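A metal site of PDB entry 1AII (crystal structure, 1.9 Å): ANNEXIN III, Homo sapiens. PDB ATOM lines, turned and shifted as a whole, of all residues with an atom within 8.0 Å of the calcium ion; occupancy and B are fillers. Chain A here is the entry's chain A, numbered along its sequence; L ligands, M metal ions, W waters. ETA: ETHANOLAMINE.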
ATOM      1  N   LEU A 182      28.826  24.459  19.967  1.00  0.00           N
ATOM      2  CA  LEU A 182      28.365  23.850  21.223  1.00  0.00           C
ATOM      3  C   LEU A 182      26.831  23.824  21.215  1.00  0.00           C
ATOM      4  O   LEU A 182      26.164  22.867  21.590  1.00  0.00           O
ATOM      5  CB  LEU A 182      28.874  24.619  22.439  1.00  0.00           C
ATOM      6  CG  LEU A 182      30.343  24.454  22.886  1.00  0.00           C
ATOM      7  CD1 LEU A 182      30.625  25.279  24.136  1.00  0.00           C
ATOM      8  CD2 LEU A 182      30.697  22.993  23.120  1.00  0.00           C
ATOM      9  N   TYR A 183      26.234  24.937  20.809  1.00  0.00           N
ATOM     10  CA  TYR A 183      24.782  25.081  20.737  1.00  0.00           C
ATOM     11  C   TYR A 183      24.190  24.041  19.784  1.00  0.00           C
ATOM     12  O   TYR A 183      23.197  23.398  20.139  1.00  0.00           O
ATOM     13  CB  TYR A 183      24.356  26.483  20.318  1.00  0.00           C
ATOM     14  CG  TYR A 183      22.865  26.715  20.351  1.00  0.00           C
ATOM     15  CD1 TYR A 183      22.186  26.840  21.565  1.00  0.00           C
ATOM     16  CD2 TYR A 183      22.122  26.826  19.183  1.00  0.00           C
ATOM     17  CE1 TYR A 183      20.828  27.061  21.603  1.00  0.00           C
ATOM     18  CE2 TYR A 183      20.750  27.034  19.209  1.00  0.00           C
ATOM     19  CZ  TYR A 183      20.101  27.150  20.423  1.00  0.00           C
ATOM     20  OH  TYR A 183      18.737  27.354  20.452  1.00  0.00           O
ATOM     21  N   LYS A 184      24.749  23.839  18.612  1.00  0.00           N
ATOM     22  CA  LYS A 184      24.277  22.880  17.631  1.00  0.00           C
ATOM     23  C   LYS A 184      24.497  21.448  18.100  1.00  0.00           C
ATOM     24  O   LYS A 184      23.706  20.574  17.749  1.00  0.00           O
ATOM     25  CB  LYS A 184      24.987  23.005  16.273  1.00  0.00           C
ATOM     26  CG  LYS A 184      24.589  24.224  15.465  1.00  0.00           C
ATOM     27  CD  LYS A 184      25.197  24.229  14.061  1.00  0.00           C
ATOM     28  CE  LYS A 184      25.185  25.636  13.489  1.00  0.00           C
ATOM     29  NZ  LYS A 184      26.253  25.860  12.464  1.00  0.00           N
ATOM     30  N   ALA A 185      25.564  21.227  18.865  1.00  0.00           N
ATOM     31  CA  ALA A 185      25.915  19.920  19.373  1.00  0.00           C
ATOM     32  C   ALA A 185      25.074  19.393  20.525  1.00  0.00           C
ATOM     33  O   ALA A 185      25.055  18.195  20.802  1.00  0.00           O
ATOM     34  CB  ALA A 185      27.378  19.996  19.878  1.00  0.00           C
ATOM     35  N   GLY A 186      24.391  20.283  21.206  1.00  0.00           N
ATOM     36  CA  GLY A 186      23.567  19.992  22.343  1.00  0.00           C
ATOM     37  C   GLY A 186      22.173  20.571  22.252  1.00  0.00           C
ATOM     38  O   GLY A 186      21.318  19.930  21.669  1.00  0.00           O
ATOM     39  N   GLU A 187      21.871  21.724  22.770  1.00  0.00           N
ATOM     40  CA  GLU A 187      20.569  22.336  22.761  1.00  0.00           C
ATOM     41  C   GLU A 187      19.790  22.243  21.469  1.00  0.00           C
ATOM     42  O   GLU A 187      18.613  21.912  21.511  1.00  0.00           O
ATOM     43  CB  GLU A 187      20.666  23.838  23.121  1.00  0.00           C
ATOM     44  CG  GLU A 187      21.156  24.082  24.531  1.00  0.00           C
ATOM     45  CD  GLU A 187      20.160  23.742  25.623  1.00  0.00           C
ATOM     46  OE1 GLU A 187      18.969  23.471  25.374  1.00  0.00           O
ATOM     47  OE2 GLU A 187      20.532  23.757  26.800  1.00  0.00           O
ATOM     48  N   ASN A 188      20.412  22.557  20.344  1.00  0.00           N
ATOM     49  CA  ASN A 188      19.733  22.539  19.069  1.00  0.00           C
ATOM     50  C   ASN A 188      19.460  21.201  18.431  1.00  0.00           C
ATOM     51  O   ASN A 188      18.852  21.216  17.344  1.00  0.00           O
ATOM     52  CB  ASN A 188      20.550  23.424  18.100  1.00  0.00           C
ATOM     53  CG  ASN A 188      19.680  23.996  16.981  1.00  0.00           C
ATOM     54  OD1 ASN A 188      19.977  23.738  15.810  1.00  0.00           O
ATOM     55  ND2 ASN A 188      18.636  24.727  17.354  1.00  0.00           N
ATOM     56  N   ARG A 189      19.825  20.061  18.969  1.00  0.00           N
ATOM     57  CA  ARG A 189      19.499  18.824  18.257  1.00  0.00           C
ATOM     58  C   ARG A 189      18.923  17.767  19.159  1.00  0.00           C
ATOM     59  O   ARG A 189      19.027  17.962  20.358  1.00  0.00           O
ATOM     60  CB  ARG A 189      20.789  18.248  17.652  1.00  0.00           C
ATOM     61  CG  ARG A 189      21.935  18.076  18.638  1.00  0.00           C
ATOM     62  CD  ARG A 189      22.994  17.176  18.038  1.00  0.00           C
ATOM     63  NE  ARG A 189      22.645  15.771  18.195  1.00  0.00           N
ATOM     64  CZ  ARG A 189      23.321  14.723  17.761  1.00  0.00           C
ATOM     65  NH1 ARG A 189      24.458  14.876  17.085  1.00  0.00           N
ATOM     66  NH2 ARG A 189      22.872  13.492  17.986  1.00  0.00           N
ATOM     67  N   TRP A 190      18.352  16.692  18.651  1.00  0.00           N
ATOM     68  CA  TRP A 190      17.836  15.636  19.513  1.00  0.00           C
ATOM     69  C   TRP A 190      19.116  14.920  19.991  1.00  0.00           C
ATOM     70  O   TRP A 190      20.024  14.743  19.167  1.00  0.00           O
ATOM     71  CB  TRP A 190      16.924  14.651  18.769  1.00  0.00           C
ATOM     72  CG  TRP A 190      15.639  15.270  18.302  1.00  0.00           C
ATOM     73  CD1 TRP A 190      15.063  16.418  18.728  1.00  0.00           C
ATOM     74  CD2 TRP A 190      14.765  14.732  17.299  1.00  0.00           C
ATOM     75  NE1 TRP A 190      13.902  16.650  18.048  1.00  0.00           N
ATOM     76  CE2 TRP A 190      13.701  15.622  17.167  1.00  0.00           C
ATOM     77  CE3 TRP A 190      14.821  13.577  16.504  1.00  0.00           C
ATOM     78  CZ2 TRP A 190      12.646  15.421  16.261  1.00  0.00           C
ATOM     79  CZ3 TRP A 190      13.782  13.373  15.617  1.00  0.00           C
ATOM     80  CH2 TRP A 190      12.715  14.275  15.510  1.00  0.00           C
ATOM     81  N   GLY A 191      19.208  14.499  21.262  1.00  0.00           N
ATOM     82  CA  GLY A 191      20.474  13.885  21.616  1.00  0.00           C
ATOM     83  C   GLY A 191      21.582  14.895  21.775  1.00  0.00           C
ATOM     84  O   GLY A 191      21.337  16.099  21.883  1.00  0.00           O
ATOM     85  N   THR A 192      22.819  14.434  21.781  1.00  0.00           N
ATOM     86  CA  THR A 192      23.959  15.319  21.936  1.00  0.00           C
ATOM     87  C   THR A 192      25.191  14.818  21.198  1.00  0.00           C
ATOM     88  O   THR A 192      25.422  13.611  21.129  1.00  0.00           O
ATOM     89  CB  THR A 192      24.366  15.453  23.430  1.00  0.00           C
ATOM     90  OG1 THR A 192      23.209  15.692  24.220  1.00  0.00           O
ATOM     91  CG2 THR A 192      25.380  16.573  23.615  1.00  0.00           C
ATOM     92  N   ASP A 193      25.956  15.720  20.619  1.00  0.00           N
ATOM     93  CA  ASP A 193      27.216  15.319  20.012  1.00  0.00           C
ATOM     94  C   ASP A 193      28.302  15.453  21.075  1.00  0.00           C
ATOM     95  O   ASP A 193      29.059  16.417  21.064  1.00  0.00           O
ATOM     96  CB  ASP A 193      27.527  16.140  18.754  1.00  0.00           C
ATOM     97  CG  ASP A 193      28.765  15.617  18.035  1.00  0.00           C
ATOM     98  OD1 ASP A 193      29.474  14.761  18.622  1.00  0.00           O
ATOM     99  OD2 ASP A 193      29.033  16.060  16.905  1.00  0.00           O
ATOM    100  N   PHE A 197      31.573  18.325  22.489  1.00  0.00           N
ATOM    101  CA  PHE A 197      31.686  18.948  23.806  1.00  0.00           C
ATOM    102  C   PHE A 197      33.101  18.678  24.331  1.00  0.00           C
ATOM    103  O   PHE A 197      33.782  19.564  24.819  1.00  0.00           O
ATOM    104  CB  PHE A 197      30.633  18.452  24.804  1.00  0.00           C
ATOM    105  CG  PHE A 197      29.358  19.255  24.792  1.00  0.00           C
ATOM    106  CD1 PHE A 197      28.374  19.044  23.836  1.00  0.00           C
ATOM    107  CD2 PHE A 197      29.142  20.257  25.735  1.00  0.00           C
ATOM    108  CE1 PHE A 197      27.217  19.804  23.858  1.00  0.00           C
ATOM    109  CE2 PHE A 197      27.990  21.020  25.748  1.00  0.00           C
ATOM    110  CZ  PHE A 197      27.019  20.798  24.807  1.00  0.00           C
ATOM    111  N   SER A 227      23.257  23.914  30.033  1.00  0.00           N
ATOM    112  CA  SER A 227      23.182  23.041  28.860  1.00  0.00           C
ATOM    113  C   SER A 227      23.842  21.704  29.161  1.00  0.00           C
ATOM    114  O   SER A 227      23.353  20.643  28.780  1.00  0.00           O
ATOM    115  CB  SER A 227      23.786  23.689  27.619  1.00  0.00           C
ATOM    116  OG  SER A 227      23.054  24.834  27.214  1.00  0.00           O
ATOM    117  N   GLY A 230      21.530  19.817  31.186  1.00  0.00           N
ATOM    118  CA  GLY A 230      20.337  19.242  30.596  1.00  0.00           C
ATOM    119  C   GLY A 230      20.652  18.248  29.506  1.00  0.00           C
ATOM    120  O   GLY A 230      19.802  17.428  29.133  1.00  0.00           O
ATOM    121  N   GLU A 231      21.880  18.290  28.990  1.00  0.00           N
ATOM    122  CA  GLU A 231      22.286  17.425  27.886  1.00  0.00           C
ATOM    123  C   GLU A 231      23.008  16.156  28.313  1.00  0.00           C
ATOM    124  O   GLU A 231      22.812  15.088  27.738  1.00  0.00           O
ATOM    125  CB  GLU A 231      23.237  18.150  26.941  1.00  0.00           C
ATOM    126  CG  GLU A 231      22.608  19.297  26.190  1.00  0.00           C
ATOM    127  CD  GLU A 231      21.666  18.823  25.105  1.00  0.00           C
ATOM    128  OE1 GLU A 231      22.021  17.875  24.380  1.00  0.00           O
ATOM    129  OE2 GLU A 231      20.561  19.404  24.985  1.00  0.00           O
ATOM    130  N   LEU A 232      23.863  16.256  29.318  1.00  0.00           N
ATOM    131  CA  LEU A 232      24.663  15.103  29.718  1.00  0.00           C
ATOM    132  C   LEU A 232      24.297  14.616  31.111  1.00  0.00           C
ATOM    133  O   LEU A 232      23.445  15.180  31.781  1.00  0.00           O
ATOM    134  CB  LEU A 232      26.133  15.476  29.592  1.00  0.00           C
ATOM    135  CG  LEU A 232      26.507  16.287  28.339  1.00  0.00           C
ATOM    136  CD1 LEU A 232      27.718  17.175  28.601  1.00  0.00           C
ATOM    137  CD2 LEU A 232      26.760  15.368  27.162  1.00  0.00           C
HETATM  138  CA  ETA L   1      21.781  11.045  21.662  1.00  0.00           C
HETATM  139  N   ETA L   1      21.777  10.778  20.196  1.00  0.00           N
HETATM  140  C   ETA L   1      20.935  10.047  22.414  1.00  0.00           C
HETATM  141  O   ETA L   1      20.727   8.907  21.596  1.00  0.00           O
HETATM  142 CA    CA M   1      20.010  17.920  22.726  1.00  0.00          CA
HETATM  143  O   HOH W   1      18.877  16.048  24.272  1.00  0.00           O
HETATM  144  O   HOH W   2      17.816  19.500  22.850  1.00  0.00           O
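The calcium ion is bound by O of Gly 191 (2.4 Å), O of Arg 189 (2.6 Å), OE1 of Glu 231 (2.6 Å), O of Gly 186 (2.6 Å), water W1 (2.7 Å), water W2 (2.7 Å) and OE2 of Glu 231 (2.8 Å).
The calcium ion has seven donor atoms within binding distance.
OE1 of Glu 231 lies close to OG1 of Thr 192 (2.5 Å).
The backbone NH (N) of Glu 187 sits close to the side-chain carboxylate (OE2) of Glu 231 (3.5 Å).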
